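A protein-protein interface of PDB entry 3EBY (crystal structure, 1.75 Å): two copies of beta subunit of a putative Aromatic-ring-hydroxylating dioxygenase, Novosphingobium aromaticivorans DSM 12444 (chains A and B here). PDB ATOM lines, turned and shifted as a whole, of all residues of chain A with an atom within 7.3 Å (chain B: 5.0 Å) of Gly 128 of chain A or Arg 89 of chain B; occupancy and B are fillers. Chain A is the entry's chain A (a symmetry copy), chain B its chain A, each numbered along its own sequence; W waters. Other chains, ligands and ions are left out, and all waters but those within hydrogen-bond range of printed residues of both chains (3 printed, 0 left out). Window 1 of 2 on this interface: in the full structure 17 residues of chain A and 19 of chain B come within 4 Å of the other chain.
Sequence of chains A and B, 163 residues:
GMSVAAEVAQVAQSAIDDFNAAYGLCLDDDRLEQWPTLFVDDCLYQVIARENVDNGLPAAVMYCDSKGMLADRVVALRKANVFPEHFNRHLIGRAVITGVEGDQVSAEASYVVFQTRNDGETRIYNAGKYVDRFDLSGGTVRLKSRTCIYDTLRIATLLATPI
The backbone carbonyl oxygen of Tyr 150 of chain A sits at hydrogen-bond distance from the backbone NH of Arg 50 of chain A, 2.9 Å away.
The guanidinium group (NE) of Arg 50 of chain A is in salt-bridge range of the side-chain carboxylate (OD1) of Asp 151 of chain A (2.8 Å).
O of Lys 129 of chain A lies within hydrogen-bond range of N of Ile 149 of chain A (2.9 Å).
O of Val 112 of chain B sits at hydrogen-bond distance from N of Leu 91 of chain B, at 3.0 Å.
The backbone NH of Phe 114 of chain B lies within hydrogen-bond range of the backbone carbonyl oxygen of Arg 89 of chain B (2.8 Å).
The backbone carbonyl oxygen (O) of Val 112 of chain A lies within hydrogen-bond range of the backbone NH (N) of Leu 91 of chain A, at 3.0 Å.
The guanidinium group (NH2) of Arg 89 of chain B lies close to the guanidinium group (NH2) of Arg 50 of chain A (3.0 Å).
The backbone carbonyl oxygen (O) of Asp 28 of chain B lies within hydrogen-bond range of the guanidinium group (NH1) of Arg 50 of chain A (2.9 Å).
NH2 of Arg 89 of chain B is in salt-bridge range of OD2 of Asp 151 of chain A.
NE of Arg 89 of chain B sits at hydrogen-bond distance from O of Gly 128 of chain A, 3.3 Å away.
NH2 of Arg 50 of chain A is in hydrogen-bond range of O of Asn 88 of chain B, 3.2 Å away.
The guanidinium group (NH1) of Arg 89 of chain B lies within hydrogen-bond range of the side-chain hydroxyl (OG) of Ser 110 of chain A (3.2 Å).
Among the printed residues, merely in contact across the chains: Ser 110 of chain A with His 90 of chain B (3.5 Å), Arg 50 of chain A with Phe 87 of chain B (3.5 Å), Ser 110 of chain A with Leu 25 of chain B (3.6 Å), Val 112 of chain A with Leu 91 of chain B (3.7 Å), Lys 129 of chain A with Arg 89 of chain B (3.7 Å), Ser 110 of chain A with Leu 91 of chain B (3.8 Å), Leu 91 of chain A with Leu 91 of chain B (3.8 Å), Ser 110 of chain A with Asp 28 of chain B (3.8 Å), Val 112 of chain A with Phe 114 of chain B (3.8 Å), Asp 151 of chain A with Phe 87 of chain B (3.9 Å) and Lys 129 of chain A with Leu 25 of chain B (3.99 Å).
Of the 18 printed residues of chain A, 7 touch a printed residue of chain B.
Hydrophobic or aromatic side chains of chain A that line the printed part of chain B: Leu 91 and Val 112.
Of the 10 printed residues of chain B, 8 touch a printed residue of chain A.
Printed residues of chain B that touch a printed residue of chain A: Leu 25, Asp 28, Phe 87, Asn 88, Arg 89, His 90, Leu 91 and Phe 114.
Among the printed residues, 17 pairs touch across the chains.
Among the printed residues, Asp or Glu carboxylates within 4 Å of a Lys or Arg side-chain nitrogen of the other chain: Asp 151 of chain A with Arg 89 of chain B.
Of the printed residues of chain B, Gly 128 of chain A touches Arg 89 (3.3 Å).
Of the printed residues of chain B, Arg 50 of chain A touches Asp 28, Phe 87, Asn 88 and Arg 89.
Printed residues of chain B within 4 Å of Val 112 of chain A: Leu 91 (3.7 Å) and Phe 114 (3.8 Å).
Printed residues of chain A within 4 Å of His 90 of chain B: Ser 110 (3.5 Å).
Thr 152 of chain A touches none of the printed residues of chain B.
Tyr 130 of chain A touches none of the printed residues of chain B.
The nearest printed residue of chain A that does not touch Arg 89 of chain B is Val 112 of chain A (4.2 Å).
Leu 91 of chain B touches its own counterpart, Leu 91 of chain A.
Val 112 of chain A touches Leu 91 of chain B, but with the chains exchanged Leu 91 of chain A does not touch Val 112 of chain B (7.4 Å).
Water W2 lies within hydrogen-bond range of the side-chain carboxylate (OD1) of Asp 151 of chain A (2.7 Å), the guanidinium group (NH2) of Arg 89 of chain B (2.7 Å) and the backbone carbonyl oxygen (O) of Ile 149 of chain A (2.7 Å).
Water W1 lies within hydrogen-bond range of OD2 of Asp 28 of chain B (2.7 Å), OG of Ser 110 of chain A (2.7 Å) and O of His 90 of chain B (2.8 Å).
Water W3 lies within hydrogen-bond range of OD2 of Asp 151 of chain A (2.9 Å) and O of Phe 87 of chain B (3.0 Å).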
ATOM      1  N   ARG A  50     -14.529   1.186  27.359  1.00  0.00           N
ATOM      2  CA  ARG A  50     -13.739   2.355  27.787  1.00  0.00           C
ATOM      3  C   ARG A  50     -13.850   2.576  29.310  1.00  0.00           C
ATOM      4  O   ARG A  50     -12.854   2.819  29.989  1.00  0.00           O
ATOM      5  CB  ARG A  50     -14.216   3.616  27.048  1.00  0.00           C
ATOM      6  CG  ARG A  50     -13.355   4.868  27.321  1.00  0.00           C
ATOM      7  CD  ARG A  50     -14.066   6.177  26.921  1.00  0.00           C
ATOM      8  NE  ARG A  50     -14.113   6.447  25.471  1.00  0.00           N
ATOM      9  CZ  ARG A  50     -13.473   7.458  24.860  1.00  0.00           C
ATOM     10  NH1 ARG A  50     -12.611   8.232  25.530  1.00  0.00           N
ATOM     11  NH2 ARG A  50     -13.640   7.653  23.561  1.00  0.00           N
ATOM     12  N   LEU A  91     -12.583   0.788   9.302  1.00  0.00           N
ATOM     13  CA  LEU A  91     -11.725   1.894   8.983  1.00  0.00           C
ATOM     14  C   LEU A  91     -10.825   2.148  10.193  1.00  0.00           C
ATOM     15  O   LEU A  91     -11.302   2.339  11.315  1.00  0.00           O
ATOM     16  CB  LEU A  91     -12.495   3.162   8.581  1.00  0.00           C
ATOM     17  CG  LEU A  91     -13.294   3.139   7.256  1.00  0.00           C
ATOM     18  CD1 LEU A  91     -14.043   4.466   7.141  1.00  0.00           C
ATOM     19  CD2 LEU A  91     -12.402   2.987   6.028  1.00  0.00           C
ATOM     20  N   ALA A 109      -4.290   3.414  17.774  1.00  0.00           N
ATOM     21  CA  ALA A 109      -4.973   3.843  16.551  1.00  0.00           C
ATOM     22  C   ALA A 109      -6.480   3.749  16.739  1.00  0.00           C
ATOM     23  O   ALA A 109      -6.985   2.743  17.262  1.00  0.00           O
ATOM     24  CB  ALA A 109      -4.518   2.983  15.367  1.00  0.00           C
ATOM     25  N   SER A 110      -7.198   4.809  16.360  1.00  0.00           N
ATOM     26  CA  SER A 110      -8.647   4.807  16.393  1.00  0.00           C
ATOM     27  C   SER A 110      -9.178   3.899  15.312  1.00  0.00           C
ATOM     28  O   SER A 110      -8.538   3.711  14.292  1.00  0.00           O
ATOM     29  CB  SER A 110      -9.227   6.218  16.191  1.00  0.00           C
ATOM     30  OG  SER A 110      -8.917   7.019  17.320  1.00  0.00           O
ATOM     31  N   TYR A 111     -10.341   3.322  15.564  1.00  0.00           N
ATOM     32  CA  TYR A 111     -11.033   2.470  14.583  1.00  0.00           C
ATOM     33  C   TYR A 111     -12.553   2.554  14.719  1.00  0.00           C
ATOM     34  O   TYR A 111     -13.095   2.854  15.792  1.00  0.00           O
ATOM     35  CB  TYR A 111     -10.590   0.994  14.722  1.00  0.00           C
ATOM     36  CG  TYR A 111     -11.161   0.310  15.968  1.00  0.00           C
ATOM     37  CD1 TYR A 111     -12.478  -0.149  16.001  1.00  0.00           C
ATOM     38  CD2 TYR A 111     -10.407   0.213  17.135  1.00  0.00           C
ATOM     39  CE1 TYR A 111     -13.009  -0.715  17.166  1.00  0.00           C
ATOM     40  CE2 TYR A 111     -10.972  -0.308  18.333  1.00  0.00           C
ATOM     41  CZ  TYR A 111     -12.265  -0.757  18.330  1.00  0.00           C
ATOM     42  OH  TYR A 111     -12.848  -1.232  19.497  1.00  0.00           O
ATOM     43  N   VAL A 112     -13.227   2.258  13.617  1.00  0.00           N
ATOM     44  CA  VAL A 112     -14.658   2.021  13.634  1.00  0.00           C
ATOM     45  C   VAL A 112     -14.923   0.823  12.783  1.00  0.00           C
ATOM     46  O   VAL A 112     -14.403   0.722  11.666  1.00  0.00           O
ATOM     47  CB  VAL A 112     -15.484   3.220  13.156  1.00  0.00           C
ATOM     48  CG1 VAL A 112     -16.974   2.849  13.149  1.00  0.00           C
ATOM     49  CG2 VAL A 112     -15.254   4.443  14.087  1.00  0.00           C
ATOM     50  N   VAL A 113     -15.718  -0.099  13.319  1.00  0.00           N
ATOM     51  CA  VAL A 113     -16.194  -1.245  12.578  1.00  0.00           C
ATOM     52  C   VAL A 113     -17.657  -0.980  12.231  1.00  0.00           C
ATOM     53  O   VAL A 113     -18.478  -0.673  13.113  1.00  0.00           O
ATOM     54  CB  VAL A 113     -16.127  -2.591  13.396  1.00  0.00           C
ATOM     55  CG1 VAL A 113     -16.660  -3.734  12.525  1.00  0.00           C
ATOM     56  CG2 VAL A 113     -14.723  -2.858  13.884  1.00  0.00           C
ATOM     57  N   ASN A 126     -19.046  -1.097  16.217  1.00  0.00           N
ATOM     58  CA  ASN A 126     -18.127  -0.912  17.341  1.00  0.00           C
ATOM     59  C   ASN A 126     -17.100   0.150  16.997  1.00  0.00           C
ATOM     60  O   ASN A 126     -16.415   0.034  15.960  1.00  0.00           O
ATOM     61  CB  ASN A 126     -17.432  -2.253  17.675  1.00  0.00           C
ATOM     62  CG  ASN A 126     -16.609  -2.191  18.915  1.00  0.00           C
ATOM     63  OD1 ASN A 126     -15.429  -1.858  18.860  1.00  0.00           O
ATOM     64  ND2 ASN A 126     -17.243  -2.438  20.079  1.00  0.00           N
ATOM     65  N   ALA A 127     -17.074   1.228  17.786  1.00  0.00           N
ATOM     66  CA  ALA A 127     -16.042   2.279  17.684  1.00  0.00           C
ATOM     67  C   ALA A 127     -15.144   2.251  18.908  1.00  0.00           C
ATOM     68  O   ALA A 127     -15.626   2.073  20.041  1.00  0.00           O
ATOM     69  CB  ALA A 127     -16.705   3.694  17.539  1.00  0.00           C
ATOM     70  N   GLY A 128     -13.848   2.505  18.709  1.00  0.00           N
ATOM     71  CA  GLY A 128     -12.881   2.445  19.823  1.00  0.00           C
ATOM     72  C   GLY A 128     -11.490   2.859  19.407  1.00  0.00           C
ATOM     73  O   GLY A 128     -11.324   3.511  18.379  1.00  0.00           O
ATOM     74  N   LYS A 129     -10.488   2.442  20.180  1.00  0.00           N
ATOM     75  CA  LYS A 129      -9.123   2.565  19.772  1.00  0.00           C
ATOM     76  C   LYS A 129      -8.343   1.313  20.150  1.00  0.00           C
ATOM     77  O   LYS A 129      -8.689   0.628  21.135  1.00  0.00           O
ATOM     78  CB  LYS A 129      -8.454   3.797  20.365  1.00  0.00           C
ATOM     79  CG  LYS A 129      -8.213   3.740  21.842  1.00  0.00           C
ATOM     80  CD  LYS A 129      -7.297   4.875  22.276  1.00  0.00           C
ATOM     81  CE  LYS A 129      -7.178   4.941  23.778  1.00  0.00           C
ATOM     82  NZ  LYS A 129      -6.135   5.967  24.209  1.00  0.00           N
ATOM     83  N   TYR A 130      -7.450   0.922  19.255  1.00  0.00           N
ATOM     84  CA  TYR A 130      -6.450  -0.121  19.566  1.00  0.00           C
ATOM     85  C   TYR A 130      -5.329   0.470  20.413  1.00  0.00           C
ATOM     86  O   TYR A 130      -4.788   1.529  20.079  1.00  0.00           O
ATOM     87  CB  TYR A 130      -5.846  -0.709  18.276  1.00  0.00           C
ATOM     88  CG  TYR A 130      -6.829  -1.318  17.302  1.00  0.00           C
ATOM     89  CD1 TYR A 130      -7.681  -2.361  17.689  1.00  0.00           C
ATOM     90  CD2 TYR A 130      -6.890  -0.880  15.978  1.00  0.00           C
ATOM     91  CE1 TYR A 130      -8.510  -3.018  16.754  1.00  0.00           C
ATOM     92  CE2 TYR A 130      -7.767  -1.476  15.037  1.00  0.00           C
ATOM     93  CZ  TYR A 130      -8.525  -2.575  15.405  1.00  0.00           C
ATOM     94  OH  TYR A 130      -9.405  -3.136  14.470  1.00  0.00           O
ATOM     95  N   CYS A 148      -8.603  -3.656  22.533  1.00  0.00           N
ATOM     96  CA  CYS A 148      -9.579  -2.854  21.798  1.00  0.00           C
ATOM     97  C   CYS A 148     -10.472  -2.188  22.814  1.00  0.00           C
ATOM     98  O   CYS A 148     -11.293  -2.859  23.475  1.00  0.00           O
ATOM     99  CB  CYS A 148     -10.427  -3.760  20.883  1.00  0.00           C
ATOM    100  SG  CYS A 148      -9.479  -4.863  19.788  1.00  0.00           S
ATOM    101  N   ILE A 149     -10.206  -0.906  23.066  1.00  0.00           N
ATOM    102  CA  ILE A 149     -10.948  -0.136  24.081  1.00  0.00           C
ATOM    103  C   ILE A 149     -12.151   0.564  23.406  1.00  0.00           C
ATOM    104  O   ILE A 149     -11.965   1.486  22.581  1.00  0.00           O
ATOM    105  CB  ILE A 149     -10.034   0.939  24.770  1.00  0.00           C
ATOM    106  CG1 ILE A 149      -8.780   0.296  25.376  1.00  0.00           C
ATOM    107  CG2 ILE A 149     -10.853   1.712  25.850  1.00  0.00           C
ATOM    108  CD1 ILE A 149      -7.863   1.271  26.111  1.00  0.00           C
ATOM    109  N   TYR A 150     -13.369   0.071  23.669  1.00  0.00           N
ATOM    110  CA  TYR A 150     -14.508   0.427  22.832  1.00  0.00           C
ATOM    111  C   TYR A 150     -15.592   1.257  23.532  1.00  0.00           C
ATOM    112  O   TYR A 150     -15.774   1.193  24.770  1.00  0.00           O
ATOM    113  CB  TYR A 150     -15.116  -0.822  22.162  1.00  0.00           C
ATOM    114  CG  TYR A 150     -15.886  -1.727  23.137  1.00  0.00           C
ATOM    115  CD1 TYR A 150     -17.233  -1.520  23.385  1.00  0.00           C
ATOM    116  CD2 TYR A 150     -15.247  -2.768  23.807  1.00  0.00           C
ATOM    117  CE1 TYR A 150     -17.935  -2.340  24.276  1.00  0.00           C
ATOM    118  CE2 TYR A 150     -15.953  -3.598  24.703  1.00  0.00           C
ATOM    119  CZ  TYR A 150     -17.274  -3.353  24.950  1.00  0.00           C
ATOM    120  OH  TYR A 150     -17.974  -4.183  25.825  1.00  0.00           O
ATOM    121  N   ASP A 151     -16.278   2.054  22.722  1.00  0.00           N
ATOM    122  CA  ASP A 151     -17.292   2.992  23.191  1.00  0.00           C
ATOM    123  C   ASP A 151     -18.716   2.406  23.115  1.00  0.00           C
ATOM    124  O   ASP A 151     -19.507   2.598  24.022  1.00  0.00           O
ATOM    125  CB  ASP A 151     -17.219   4.290  22.355  1.00  0.00           C
ATOM    126  CG  ASP A 151     -15.920   5.025  22.542  1.00  0.00           C
ATOM    127  OD1 ASP A 151     -15.226   4.732  23.555  1.00  0.00           O
ATOM    128  OD2 ASP A 151     -15.569   5.832  21.649  1.00  0.00           O
ATOM    129  N   THR A 152     -18.992   1.662  22.047  1.00  0.00           N
ATOM    130  CA  THR A 152     -20.340   1.217  21.685  1.00  0.00           C
ATOM    131  C   THR A 152     -20.828   0.103  22.625  1.00  0.00           C
ATOM    132  O   THR A 152     -20.174  -0.928  22.752  1.00  0.00           O
ATOM    133  CB  THR A 152     -20.359   0.705  20.241  1.00  0.00           C
ATOM    134  OG1 THR A 152     -19.602   1.606  19.398  1.00  0.00           O
ATOM    135  CG2 THR A 152     -21.809   0.573  19.702  1.00  0.00           C
ATOM    136  N   ILE A 163     -12.606  -7.911  16.642  1.00  0.00           N
ATOM    137  CA  ILE A 163     -12.520  -6.482  16.374  1.00  0.00           C
ATOM    138  C   ILE A 163     -11.105  -6.162  15.911  1.00  0.00           C
ATOM    139  O   ILE A 163     -10.906  -5.414  14.946  1.00  0.00           O
ATOM    140  CB  ILE A 163     -12.856  -5.619  17.645  1.00  0.00           C
ATOM    141  CG1 ILE A 163     -14.253  -5.920  18.167  1.00  0.00           C
ATOM    142  CG2 ILE A 163     -12.756  -4.103  17.336  1.00  0.00           C
ATOM    143  CD1 ILE A 163     -15.335  -5.608  17.151  1.00  0.00           C
ATOM    144  OXT ILE A 163     -10.120  -6.685  16.472  1.00  0.00           O
ATOM    145  N   LEU B  25      -6.593  11.830  18.585  1.00  0.00           N
ATOM    146  CA  LEU B  25      -6.481  11.025  19.821  1.00  0.00           C
ATOM    147  C   LEU B  25      -6.495  11.912  21.072  1.00  0.00           C
ATOM    148  O   LEU B  25      -7.095  11.546  22.080  1.00  0.00           O
ATOM    149  CB  LEU B  25      -5.242  10.126  19.804  1.00  0.00           C
ATOM    150  CG  LEU B  25      -5.465   8.751  19.130  1.00  0.00           C
ATOM    151  CD1 LEU B  25      -4.163   7.963  19.099  1.00  0.00           C
ATOM    152  CD2 LEU B  25      -6.565   7.951  19.839  1.00  0.00           C
ATOM    153  N   ASP B  28     -10.192  12.696  21.602  1.00  0.00           N
ATOM    154  CA  ASP B  28     -10.961  11.489  21.927  1.00  0.00           C
ATOM    155  C   ASP B  28     -10.628  10.956  23.327  1.00  0.00           C
ATOM    156  O   ASP B  28     -11.504  10.440  24.017  1.00  0.00           O
ATOM    157  CB  ASP B  28     -10.702  10.416  20.915  1.00  0.00           C
ATOM    158  CG  ASP B  28     -11.193  10.786  19.515  1.00  0.00           C
ATOM    159  OD1 ASP B  28     -11.984  11.761  19.376  1.00  0.00           O
ATOM    160  OD2 ASP B  28     -10.768  10.099  18.567  1.00  0.00           O
ATOM    161  N   PHE B  87     -18.701  10.123  24.718  1.00  0.00           N
ATOM    162  CA  PHE B  87     -17.441   9.584  24.244  1.00  0.00           C
ATOM    163  C   PHE B  87     -17.332   9.870  22.757  1.00  0.00           C
ATOM    164  O   PHE B  87     -18.235   9.527  21.985  1.00  0.00           O
ATOM    165  CB  PHE B  87     -17.354   8.085  24.473  1.00  0.00           C
ATOM    166  CG  PHE B  87     -17.372   7.693  25.921  1.00  0.00           C
ATOM    167  CD1 PHE B  87     -16.839   8.529  26.891  1.00  0.00           C
ATOM    168  CD2 PHE B  87     -17.902   6.472  26.315  1.00  0.00           C
ATOM    169  CE1 PHE B  87     -16.877   8.169  28.229  1.00  0.00           C
ATOM    170  CE2 PHE B  87     -17.899   6.100  27.650  1.00  0.00           C
ATOM    171  CZ  PHE B  87     -17.399   6.960  28.600  1.00  0.00           C
ATOM    172  N   ASN B  88     -16.212  10.468  22.374  1.00  0.00           N
ATOM    173  CA  ASN B  88     -15.967  10.836  20.990  1.00  0.00           C
ATOM    174  C   ASN B  88     -14.897   9.991  20.366  1.00  0.00           C
ATOM    175  O   ASN B  88     -13.942   9.568  21.031  1.00  0.00           O
ATOM    176  CB  ASN B  88     -15.577  12.305  20.886  1.00  0.00           C
ATOM    177  CG  ASN B  88     -16.692  13.230  21.314  1.00  0.00           C
ATOM    178  OD1 ASN B  88     -17.822  13.142  20.801  1.00  0.00           O
ATOM    179  ND2 ASN B  88     -16.444  13.992  22.376  1.00  0.00           N
ATOM    180  N   ARG B  89     -15.002   9.843  19.045  1.00  0.00           N
ATOM    181  CA  ARG B  89     -14.066   9.081  18.272  1.00  0.00           C
ATOM    182  C   ARG B  89     -13.890   9.787  16.926  1.00  0.00           C
ATOM    183  O   ARG B  89     -14.855   9.928  16.179  1.00  0.00           O
ATOM    184  CB  ARG B  89     -14.647   7.684  18.036  1.00  0.00           C
ATOM    185  CG  ARG B  89     -13.771   6.760  17.291  1.00  0.00           C
ATOM    186  CD  ARG B  89     -12.509   6.561  18.030  1.00  0.00           C
ATOM    187  NE  ARG B  89     -12.745   6.267  19.443  1.00  0.00           N
ATOM    188  CZ  ARG B  89     -11.808   6.386  20.372  1.00  0.00           C
ATOM    189  NH1 ARG B  89     -10.605   6.810  20.049  1.00  0.00           N
ATOM    190  NH2 ARG B  89     -12.064   6.059  21.614  1.00  0.00           N
ATOM    191  N   HIS B  90     -12.663  10.197  16.618  1.00  0.00           N
ATOM    192  CA  HIS B  90     -12.330  10.795  15.300  1.00  0.00           C
ATOM    193  C   HIS B  90     -11.706   9.735  14.386  1.00  0.00           C
ATOM    194  O   HIS B  90     -10.806   8.977  14.806  1.00  0.00           O
ATOM    195  CB  HIS B  90     -11.267  11.902  15.440  1.00  0.00           C
ATOM    196  CG  HIS B  90     -11.770  13.202  15.988  1.00  0.00           C
ATOM    197  ND1 HIS B  90     -12.122  13.362  17.311  1.00  0.00           N
ATOM    198  CD2 HIS B  90     -11.727  14.457  15.459  1.00  0.00           C
ATOM    199  CE1 HIS B  90     -12.425  14.633  17.533  1.00  0.00           C
ATOM    200  NE2 HIS B  90     -12.221  15.318  16.415  1.00  0.00           N
ATOM    201  N   LEU B  91     -12.156   9.706  13.137  1.00  0.00           N
ATOM    202  CA  LEU B  91     -11.383   9.127  12.076  1.00  0.00           C
ATOM    203  C   LEU B  91     -11.041  10.243  11.087  1.00  0.00           C
ATOM    204  O   LEU B  91     -11.924  10.944  10.586  1.00  0.00           O
ATOM    205  CB  LEU B  91     -12.095   7.958  11.376  1.00  0.00           C
ATOM    206  CG  LEU B  91     -12.328   6.659  12.185  1.00  0.00           C
ATOM    207  CD1 LEU B  91     -13.136   5.704  11.308  1.00  0.00           C
ATOM    208  CD2 LEU B  91     -11.030   5.964  12.580  1.00  0.00           C
ATOM    209  N   VAL B 112     -14.546  12.362  10.234  1.00  0.00           N
ATOM    210  CA  VAL B 112     -15.839  12.106  10.841  1.00  0.00           C
ATOM    211  C   VAL B 112     -15.617  11.927  12.306  1.00  0.00           C
ATOM    212  O   VAL B 112     -14.707  11.196  12.717  1.00  0.00           O
ATOM    213  CB  VAL B 112     -16.565  10.894  10.249  1.00  0.00           C
ATOM    214  CG1 VAL B 112     -17.885  10.668  10.999  1.00  0.00           C
ATOM    215  CG2 VAL B 112     -16.852  11.117   8.738  1.00  0.00           C
ATOM    216  N   VAL B 113     -16.436  12.611  13.101  1.00  0.00           N
ATOM    217  CA  VAL B 113     -16.455  12.440  14.535  1.00  0.00           C
ATOM    218  C   VAL B 113     -17.701  11.625  14.874  1.00  0.00           C
ATOM    219  O   VAL B 113     -18.824  11.978  14.473  1.00  0.00           O
ATOM    220  CB  VAL B 113     -16.536  13.800  15.327  1.00  0.00           C
ATOM    221  CG1 VAL B 113     -16.560  13.504  16.831  1.00  0.00           C
ATOM    222  CG2 VAL B 113     -15.397  14.716  14.948  1.00  0.00           C
ATOM    223  N   PHE B 114     -17.466  10.505  15.502  1.00  0.00           N
ATOM    224  CA  PHE B 114     -18.515   9.604  15.995  1.00  0.00           C
ATOM    225  C   PHE B 114     -18.689   9.835  17.502  1.00  0.00           C
ATOM    226  O   PHE B 114     -17.715  10.089  18.224  1.00  0.00           O
ATOM    227  CB  PHE B 114     -18.119   8.143  15.742  1.00  0.00           C
ATOM    228  CG  PHE B 114     -17.784   7.839  14.309  1.00  0.00           C
ATOM    229  CD1 PHE B 114     -16.506   8.072  13.812  1.00  0.00           C
ATOM    230  CD2 PHE B 114     -18.760   7.393  13.437  1.00  0.00           C
ATOM    231  CE1 PHE B 114     -16.205   7.835  12.486  1.00  0.00           C
ATOM    232  CE2 PHE B 114     -18.461   7.162  12.090  1.00  0.00           C
ATOM    233  CZ  PHE B 114     -17.200   7.397  11.617  1.00  0.00           C
HETATM  234  O   HOH W   1      -8.903   9.653  16.701  1.00  0.00           O
HETATM  235  O   HOH W   2     -12.675   4.051  23.258  1.00  0.00           O
HETATM  236  O   HOH W   3     -17.914   6.964  20.368  1.00  0.00           O
